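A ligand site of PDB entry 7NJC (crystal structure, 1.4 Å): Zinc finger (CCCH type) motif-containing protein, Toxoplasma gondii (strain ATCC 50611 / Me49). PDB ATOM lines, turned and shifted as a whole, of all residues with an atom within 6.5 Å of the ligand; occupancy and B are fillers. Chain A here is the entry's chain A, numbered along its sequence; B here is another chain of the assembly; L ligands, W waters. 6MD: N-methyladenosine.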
ATOM      1  N   ILE A  19     -17.586 -11.578   0.870  1.00  0.00           N
ATOM      2  CA  ILE A  19     -18.206 -12.045   2.105  1.00  0.00           C
ATOM      3  C   ILE A  19     -17.111 -12.201   3.138  1.00  0.00           C
ATOM      4  O   ILE A  19     -16.086 -12.831   2.870  1.00  0.00           O
ATOM      5  CB  ILE A  19     -18.930 -13.394   1.879  1.00  0.00           C
ATOM      6  CG1 ILE A  19     -20.130 -13.204   0.942  1.00  0.00           C
ATOM      7  CG2 ILE A  19     -19.286 -14.051   3.229  1.00  0.00           C
ATOM      8  CD1 ILE A  19     -21.229 -12.272   1.479  1.00  0.00           C
ATOM      9  N   LYS A  20     -17.307 -11.606   4.319  1.00  0.00           N
ATOM     10  CA  LYS A  20     -16.377 -11.739   5.421  1.00  0.00           C
ATOM     11  C   LYS A  20     -17.012 -12.576   6.523  1.00  0.00           C
ATOM     12  O   LYS A  20     -18.222 -12.505   6.758  1.00  0.00           O
ATOM     13  CB  LYS A  20     -15.998 -10.363   5.990  1.00  0.00           C
ATOM     14  CG  LYS A  20     -15.343  -9.409   4.987  1.00  0.00           C
ATOM     15  CD  LYS A  20     -14.001  -9.911   4.457  1.00  0.00           C
ATOM     16  CE  LYS A  20     -12.963 -10.008   5.565  1.00  0.00           C
ATOM     17  NZ  LYS A  20     -11.578 -10.122   5.011  1.00  0.00           N
ATOM     18  N   SER A  21     -16.196 -13.386   7.195  1.00  0.00           N
ATOM     19  CA  SER A  21     -16.659 -14.187   8.318  1.00  0.00           C
ATOM     20  C   SER A  21     -15.722 -13.948   9.490  1.00  0.00           C
ATOM     21  O   SER A  21     -14.512 -14.009   9.322  1.00  0.00           O
ATOM     22  CB  SER A  21     -16.638 -15.683   7.984  1.00  0.00           C
ATOM     23  OG  SER A  21     -17.107 -16.423   9.103  1.00  0.00           O
ATOM     24  N   ASN A  22     -16.288 -13.694  10.676  1.00  0.00           N
ATOM     25  CA  ASN A  22     -15.412 -13.506  11.828  1.00  0.00           C
ATOM     26  C   ASN A  22     -14.987 -14.815  12.481  1.00  0.00           C
ATOM     27  O   ASN A  22     -14.200 -14.795  13.429  1.00  0.00           O
ATOM     28  CB  ASN A  22     -16.015 -12.529  12.843  1.00  0.00           C
ATOM     29  CG  ASN A  22     -17.430 -12.894  13.264  1.00  0.00           C
ATOM     30  OD1 ASN A  22     -17.791 -14.076  13.323  1.00  0.00           O
ATOM     31  ND2 ASN A  22     -18.243 -11.881  13.560  1.00  0.00           N
ATOM     32  N   ARG A  23     -15.474 -15.964  11.992  1.00  0.00           N
ATOM     33  CA  ARG A  23     -15.140 -17.249  12.590  1.00  0.00           C
ATOM     34  C   ARG A  23     -14.952 -18.267  11.469  1.00  0.00           C
ATOM     35  O   ARG A  23     -15.817 -18.409  10.603  1.00  0.00           O
ATOM     36  CB  ARG A  23     -16.250 -17.724  13.534  1.00  0.00           C
ATOM     37  CG  ARG A  23     -16.487 -16.760  14.707  1.00  0.00           C
ATOM     38  CD  ARG A  23     -17.630 -17.189  15.593  1.00  0.00           C
ATOM     39  NE  ARG A  23     -17.360 -18.475  16.199  1.00  0.00           N
ATOM     40  CZ  ARG A  23     -17.949 -18.925  17.309  1.00  0.00           C
ATOM     41  NH1 ARG A  23     -18.851 -18.184  17.937  1.00  0.00           N
ATOM     42  NH2 ARG A  23     -17.622 -20.117  17.773  1.00  0.00           N
ATOM     43  N   ASN A  26     -17.728 -20.964  10.726  1.00  0.00           N
ATOM     44  CA  ASN A  26     -18.883 -20.700   9.885  1.00  0.00           C
ATOM     45  C   ASN A  26     -18.567 -20.966   8.417  1.00  0.00           C
ATOM     46  O   ASN A  26     -19.454 -21.377   7.652  1.00  0.00           O
ATOM     47  CB  ASN A  26     -19.411 -19.292  10.121  1.00  0.00           C
ATOM     48  CG  ASN A  26     -20.105 -19.153  11.469  1.00  0.00           C
ATOM     49  OD1 ASN A  26     -20.165 -20.111  12.246  1.00  0.00           O
ATOM     50  ND2 ASN A  26     -20.631 -17.978  11.731  1.00  0.00           N
ATOM     51  N   ILE A  27     -17.327 -20.747   8.001  1.00  0.00           N
ATOM     52  CA  ILE A  27     -16.901 -21.171   6.669  1.00  0.00           C
ATOM     53  C   ILE A  27     -17.000 -22.691   6.533  1.00  0.00           C
ATOM     54  O   ILE A  27     -17.510 -23.206   5.537  1.00  0.00           O
ATOM     55  CB  ILE A  27     -15.509 -20.610   6.329  1.00  0.00           C
ATOM     56  CG1 ILE A  27     -15.609 -19.109   6.081  1.00  0.00           C
ATOM     57  CG2 ILE A  27     -14.903 -21.314   5.123  1.00  0.00           C
ATOM     58  CD1 ILE A  27     -14.304 -18.425   5.803  1.00  0.00           C
ATOM     59  N   TRP A  36     -25.355 -20.022   3.753  1.00  0.00           N
ATOM     60  CA  TRP A  36     -24.757 -18.820   4.315  1.00  0.00           C
ATOM     61  C   TRP A  36     -25.860 -17.938   4.883  1.00  0.00           C
ATOM     62  O   TRP A  36     -27.052 -18.179   4.664  1.00  0.00           O
ATOM     63  CB  TRP A  36     -23.904 -18.065   3.270  1.00  0.00           C
ATOM     64  CG  TRP A  36     -23.028 -17.024   3.899  1.00  0.00           C
ATOM     65  CD1 TRP A  36     -23.119 -15.666   3.758  1.00  0.00           C
ATOM     66  CD2 TRP A  36     -21.957 -17.266   4.815  1.00  0.00           C
ATOM     67  NE1 TRP A  36     -22.156 -15.043   4.525  1.00  0.00           N
ATOM     68  CE2 TRP A  36     -21.424 -16.002   5.180  1.00  0.00           C
ATOM     69  CE3 TRP A  36     -21.387 -18.424   5.355  1.00  0.00           C
ATOM     70  CZ2 TRP A  36     -20.353 -15.870   6.058  1.00  0.00           C
ATOM     71  CZ3 TRP A  36     -20.325 -18.291   6.237  1.00  0.00           C
ATOM     72  CH2 TRP A  36     -19.813 -17.023   6.580  1.00  0.00           C
ATOM     73  N   ALA A  37     -25.460 -16.952   5.678  1.00  0.00           N
ATOM     74  CA  ALA A  37     -26.347 -15.878   6.125  1.00  0.00           C
ATOM     75  C   ALA A  37     -25.468 -14.673   6.389  1.00  0.00           C
ATOM     76  O   ALA A  37     -24.291 -14.804   6.708  1.00  0.00           O
ATOM     77  CB  ALA A  37     -27.110 -16.233   7.403  1.00  0.00           C
ATOM     78  N   THR A  38     -26.055 -13.486   6.247  1.00  0.00           N
ATOM     79  CA  THR A  38     -25.315 -12.250   6.423  1.00  0.00           C
ATOM     80  C   THR A  38     -26.123 -11.303   7.300  1.00  0.00           C
ATOM     81  O   THR A  38     -27.219 -11.644   7.749  1.00  0.00           O
ATOM     82  CB  THR A  38     -24.902 -11.672   5.052  1.00  0.00           C
ATOM     83  OG1 THR A  38     -24.021 -10.557   5.230  1.00  0.00           O
ATOM     84  CG2 THR A  38     -26.130 -11.256   4.246  1.00  0.00           C
ATOM     85  N   SER A  39     -25.574 -10.121   7.563  1.00  0.00           N
ATOM     86  CA  SER A  39     -26.285  -9.105   8.321  1.00  0.00           C
ATOM     87  C   SER A  39     -27.615  -8.787   7.634  1.00  0.00           C
ATOM     88  O   SER A  39     -27.797  -8.994   6.440  1.00  0.00           O
ATOM     89  CB  SER A  39     -25.457  -7.831   8.414  1.00  0.00           C
ATOM     90  OG  SER A  39     -25.286  -7.259   7.123  1.00  0.00           O
ATOM     91  N   ASN A  42     -27.124  -6.469   4.650  1.00  0.00           N
ATOM     92  CA  ASN A  42     -26.548  -7.149   3.493  1.00  0.00           C
ATOM     93  C   ASN A  42     -27.495  -8.200   2.929  1.00  0.00           C
ATOM     94  O   ASN A  42     -27.419  -8.504   1.739  1.00  0.00           O
ATOM     95  CB  ASN A  42     -25.221  -7.807   3.856  1.00  0.00           C
ATOM     96  CG  ASN A  42     -24.078  -6.830   3.899  1.00  0.00           C
ATOM     97  OD1 ASN A  42     -24.113  -5.769   3.265  1.00  0.00           O
ATOM     98  ND2 ASN A  42     -23.030  -7.189   4.640  1.00  0.00           N
ATOM     99  N   SER A  61     -13.854 -14.522   2.416  1.00  0.00           N
ATOM    100  CA  SER A  61     -12.599 -14.142   3.070  1.00  0.00           C
ATOM    101  C   SER A  61     -12.823 -14.051   4.569  1.00  0.00           C
ATOM    102  O   SER A  61     -13.482 -13.112   5.042  1.00  0.00           O
ATOM    103  CB  SER A  61     -12.104 -12.805   2.527  1.00  0.00           C
ATOM    104  OG  SER A  61     -11.015 -12.311   3.291  1.00  0.00           O
ATOM    105  N   ALA A  62     -12.261 -14.987   5.330  1.00  0.00           N
ATOM    106  CA  ALA A  62     -12.357 -14.925   6.778  1.00  0.00           C
ATOM    107  C   ALA A  62     -11.558 -13.741   7.321  1.00  0.00           C
ATOM    108  O   ALA A  62     -10.485 -13.406   6.805  1.00  0.00           O
ATOM    109  CB  ALA A  62     -11.839 -16.217   7.410  1.00  0.00           C
ATOM    110  N   ASN A  63     -12.097 -13.096   8.358  1.00  0.00           N
ATOM    111  CA  ASN A  63     -11.411 -11.967   8.985  1.00  0.00           C
ATOM    112  C   ASN A  63     -10.011 -12.394   9.409  1.00  0.00           C
ATOM    113  O   ASN A  63      -9.817 -13.457  10.001  1.00  0.00           O
ATOM    114  CB  ASN A  63     -12.178 -11.503  10.226  1.00  0.00           C
ATOM    115  CG  ASN A  63     -13.474 -10.748   9.900  1.00  0.00           C
ATOM    116  OD1 ASN A  63     -13.935 -10.723   8.756  1.00  0.00           O
ATOM    117  ND2 ASN A  63     -14.068 -10.146  10.926  1.00  0.00           N
ATOM    118  N   TRP A  87     -25.932 -21.620  12.867  1.00  0.00           N
ATOM    119  CA  TRP A  87     -24.741 -20.896  13.290  1.00  0.00           C
ATOM    120  C   TRP A  87     -24.629 -20.732  14.791  1.00  0.00           C
ATOM    121  O   TRP A  87     -23.611 -20.226  15.268  1.00  0.00           O
ATOM    122  CB  TRP A  87     -24.728 -19.488  12.681  1.00  0.00           C
ATOM    123  CG  TRP A  87     -25.125 -19.460  11.252  1.00  0.00           C
ATOM    124  CD1 TRP A  87     -26.293 -18.995  10.742  1.00  0.00           C
ATOM    125  CD2 TRP A  87     -24.363 -19.944  10.144  1.00  0.00           C
ATOM    126  NE1 TRP A  87     -26.311 -19.153   9.386  1.00  0.00           N
ATOM    127  CE2 TRP A  87     -25.142 -19.742   8.987  1.00  0.00           C
ATOM    128  CE3 TRP A  87     -23.096 -20.540  10.019  1.00  0.00           C
ATOM    129  CZ2 TRP A  87     -24.690 -20.100   7.713  1.00  0.00           C
ATOM    130  CZ3 TRP A  87     -22.661 -20.895   8.754  1.00  0.00           C
ATOM    131  CH2 TRP A  87     -23.461 -20.680   7.619  1.00  0.00           C
ATOM    132  N   VAL A  90     -25.584 -16.491  17.076  1.00  0.00           N
ATOM    133  CA  VAL A  90     -25.402 -15.398  16.119  1.00  0.00           C
ATOM    134  C   VAL A  90     -26.521 -15.350  15.089  1.00  0.00           C
ATOM    135  O   VAL A  90     -26.767 -14.300  14.487  1.00  0.00           O
ATOM    136  CB  VAL A  90     -23.990 -15.425  15.481  1.00  0.00           C
ATOM    137  CG1 VAL A  90     -23.848 -16.589  14.537  1.00  0.00           C
ATOM    138  CG2 VAL A  90     -23.707 -14.105  14.760  1.00  0.00           C
ATOM    139  N   LEU A  94     -28.433 -12.144  12.391  1.00  0.00           N
ATOM    140  CA  LEU A  94     -28.269 -12.297  10.948  1.00  0.00           C
ATOM    141  C   LEU A  94     -29.642 -12.337  10.298  1.00  0.00           C
ATOM    142  O   LEU A  94     -30.665 -12.518  10.968  1.00  0.00           O
ATOM    143  CB  LEU A  94     -27.515 -13.595  10.636  1.00  0.00           C
ATOM    144  CG  LEU A  94     -26.073 -13.685  11.143  1.00  0.00           C
ATOM    145  CD1 LEU A  94     -25.543 -15.104  11.050  1.00  0.00           C
ATOM    146  CD2 LEU A  94     -25.182 -12.736  10.350  1.00  0.00           C
ATOM    147  N   ASN A  97     -31.154 -17.827   6.569  1.00  0.00           N
ATOM    148  CA  ASN A  97     -30.146 -18.572   5.812  1.00  0.00           C
ATOM    149  C   ASN A  97     -30.557 -18.734   4.364  1.00  0.00           C
ATOM    150  O   ASN A  97     -31.742 -18.843   4.030  1.00  0.00           O
ATOM    151  CB  ASN A  97     -29.961 -19.948   6.452  1.00  0.00           C
ATOM    152  CG  ASN A  97     -29.476 -19.837   7.861  1.00  0.00           C
ATOM    153  OD1 ASN A  97     -28.782 -18.869   8.205  1.00  0.00           O
ATOM    154  ND2 ASN A  97     -29.811 -20.816   8.699  1.00  0.00           N
ATOM    155  N   ARG A 130     -15.171  -4.673   3.536  1.00  0.00           N
ATOM    156  CA  ARG A 130     -16.070  -5.148   4.569  1.00  0.00           C
ATOM    157  C   ARG A 130     -17.026  -6.178   3.979  1.00  0.00           C
ATOM    158  O   ARG A 130     -17.137  -6.334   2.755  1.00  0.00           O
ATOM    159  CB  ARG A 130     -16.847  -3.981   5.193  1.00  0.00           C
ATOM    160  CG  ARG A 130     -15.964  -2.972   5.939  1.00  0.00           C
ATOM    161  CD  ARG A 130     -16.788  -1.900   6.655  1.00  0.00           C
ATOM    162  NE  ARG A 130     -17.510  -1.021   5.722  1.00  0.00           N
ATOM    163  CZ  ARG A 130     -18.832  -0.991   5.597  1.00  0.00           C
ATOM    164  NH1 ARG A 130     -19.596  -1.787   6.331  1.00  0.00           N
ATOM    165  NH2 ARG A 130     -19.386  -0.167   4.724  1.00  0.00           N
ATOM    166  N   ASP A 131     -17.720  -6.884   4.853  1.00  0.00           N
ATOM    167  CA  ASP A 131     -18.714  -7.869   4.428  1.00  0.00           C
ATOM    168  C   ASP A 131     -19.748  -7.217   3.515  1.00  0.00           C
ATOM    169  O   ASP A 131     -20.291  -6.152   3.820  1.00  0.00           O
ATOM    170  CB  ASP A 131     -19.405  -8.416   5.679  1.00  0.00           C
ATOM    171  CG  ASP A 131     -20.388  -9.535   5.360  1.00  0.00           C
ATOM    172  OD1 ASP A 131     -20.003 -10.463   4.619  1.00  0.00           O
ATOM    173  OD2 ASP A 131     -21.524  -9.487   5.891  1.00  0.00           O
ATOM    174  P     C B   4     -16.693  -6.668   8.598  1.00  0.00           P
ATOM    175  OP1   C B   4     -16.232  -5.702   9.640  1.00  0.00           O
ATOM    176  OP2   C B   4     -17.802  -6.379   7.659  1.00  0.00           O
ATOM    177  O5'   C B   4     -15.468  -7.110   7.695  1.00  0.00           O
ATOM    178  C5'   C B   4     -14.149  -7.152   8.209  1.00  0.00           C
ATOM    179  C4'   C B   4     -13.225  -6.358   7.322  1.00  0.00           C
ATOM    180  O4'   C B   4     -13.621  -4.967   7.327  1.00  0.00           O
ATOM    181  C3'   C B   4     -11.769  -6.369   7.718  1.00  0.00           C
ATOM    182  O3'   C B   4     -11.128  -7.507   7.172  1.00  0.00           O
ATOM    183  C2'   C B   4     -11.254  -5.054   7.130  1.00  0.00           C
ATOM    184  O2'   C B   4     -10.946  -5.238   5.761  1.00  0.00           O
ATOM    185  C1'   C B   4     -12.485  -4.150   7.217  1.00  0.00           C
ATOM    186  N1    C B   4     -12.498  -3.198   8.350  1.00  0.00           N
ATOM    187  C2    C B   4     -11.612  -2.123   8.389  1.00  0.00           C
ATOM    188  O2    C B   4     -10.765  -1.995   7.487  1.00  0.00           O
ATOM    189  N3    C B   4     -11.693  -1.251   9.426  1.00  0.00           N
ATOM    190  C4    C B   4     -12.621  -1.408  10.375  1.00  0.00           C
ATOM    191  N4    C B   4     -12.650  -0.523  11.377  1.00  0.00           N
ATOM    192  C5    C B   4     -13.557  -2.486  10.348  1.00  0.00           C
ATOM    193  C6    C B   4     -13.460  -3.340   9.316  1.00  0.00           C
HETATM  194  O5' 6MD L   1     -20.229  -7.159  12.166  1.00  0.00           O
HETATM  195  C5' 6MD L   1     -19.735  -7.330  10.832  1.00  0.00           C
HETATM  196  C4' 6MD L   1     -18.923  -8.608  10.727  1.00  0.00           C
HETATM  197  O4' 6MD L   1     -19.805  -9.744  10.714  1.00  0.00           O
HETATM  198  C3' 6MD L   1     -18.077  -8.800   9.524  1.00  0.00           C
HETATM  199  O3' 6MD L   1     -16.957  -8.010   9.342  1.00  0.00           O
HETATM  200  C2' 6MD L   1     -17.941 -10.253   9.392  1.00  0.00           C
HETATM  201  O2' 6MD L   1     -16.713 -10.904   9.316  1.00  0.00           O
HETATM  202  C1' 6MD L   1     -19.091 -10.842  10.170  1.00  0.00           C
HETATM  203  N9  6MD L   1     -20.055 -11.718   9.495  1.00  0.00           N
HETATM  204  C8  6MD L   1     -20.961 -11.349   8.699  1.00  0.00           C
HETATM  205  N7  6MD L   1     -21.700 -12.463   8.421  1.00  0.00           N
HETATM  206  C5  6MD L   1     -21.166 -13.506   9.153  1.00  0.00           C
HETATM  207  C6  6MD L   1     -21.430 -14.914   9.337  1.00  0.00           C
HETATM  208  N6  6MD L   1     -22.534 -15.598   8.621  1.00  0.00           N
HETATM  209  N1  6MD L   1     -20.675 -15.635  10.156  1.00  0.00           N
HETATM  210  C2  6MD L   1     -19.640 -15.052  10.830  1.00  0.00           C
HETATM  211  N3  6MD L   1     -19.364 -13.747  10.676  1.00  0.00           N
HETATM  212  C4  6MD L   1     -20.094 -12.948   9.863  1.00  0.00           C
HETATM  213  CZ  6MD L   1     -22.837 -16.942   8.984  1.00  0.00           C
HETATM  214  O   HOH W   1     -21.798 -12.394   5.356  1.00  0.00           O
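The backbone carbonyl oxygen of Lys 20 lies close to an oxygen (O2') of the ligand, 3.4 Å away. The backbone NH (N) of Ser 21 lies close to an oxygen (O2') of the ligand (3.3 Å). The backbone NH (N) of Asn 22 is in hydrogen-bond range of a nitrogen (N3) of the ligand, 3.1 Å away. P of C 4 of chain B is bonded to an oxygen (O3') of the ligand. The backbone carbonyl oxygen of Ala 37 is in hydrogen-bond range of a nitrogen (N6) of the ligand (2.7 Å). An oxygen (O2') of the ligand sits at hydrogen-bond distance from the side-chain amide oxygen of Asn 63, at 2.8 Å. The side-chain amide oxygen (OD1) of Asn 22 sits close to a nitrogen (N3) of the ligand (3.1 Å). The side-chain amide nitrogen (ND2) of Asn 26 lies within hydrogen-bond range of a nitrogen (N1) of the ligand.
OD2 of Asp 131 is in hydrogen-bond range of OG1 of Thr 38, at 2.8 Å. The side-chain amide oxygen (OD1) of Asn 97 is in hydrogen-bond range of the indole nitrogen (NE1) of Trp 87, at 2.8 Å. The side-chain amino group of Lys 20 is in hydrogen-bond range of O3' of C 4 of chain B (3.4 Å). The backbone NH (N) of Ser 21 lies within hydrogen-bond range of the backbone carbonyl oxygen (O) of Ser 61. O of Ser 21 lies within hydrogen-bond range of N of Asn 63 (2.8 Å). N of Lys 20 lies within hydrogen-bond range of OD1 of Asp 131 (2.9 Å). The side-chain carboxylate of Asp 131 sits at hydrogen-bond distance from the side-chain amide nitrogen of Asn 42. OG of Ser 61 sits at hydrogen-bond distance from NZ of Lys 20.
Merely in contact with the ligand: Trp 36, Asp 131, Trp 87 and Leu 94. Hydrophobic or aromatic side chains within 4 Å of the ligand: Trp 36, Trp 87 and Leu 94. Within 4 Å of the ligand: Lys 20, Ser 21, Asn 22, Asn 26, Trp 36, Ala 37, Asn 63, Trp 87, Leu 94, Asp 131 and C 4 of chain B. The nearest printed residue that does not touch the ligand is Thr 38 (4.1 Å).
Water W1 lies within hydrogen-bond range of the side-chain carboxylate of Asp 131, the indole nitrogen of Trp 36, the side-chain hydroxyl of Thr 38 and a nitrogen (N7) of the ligand.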
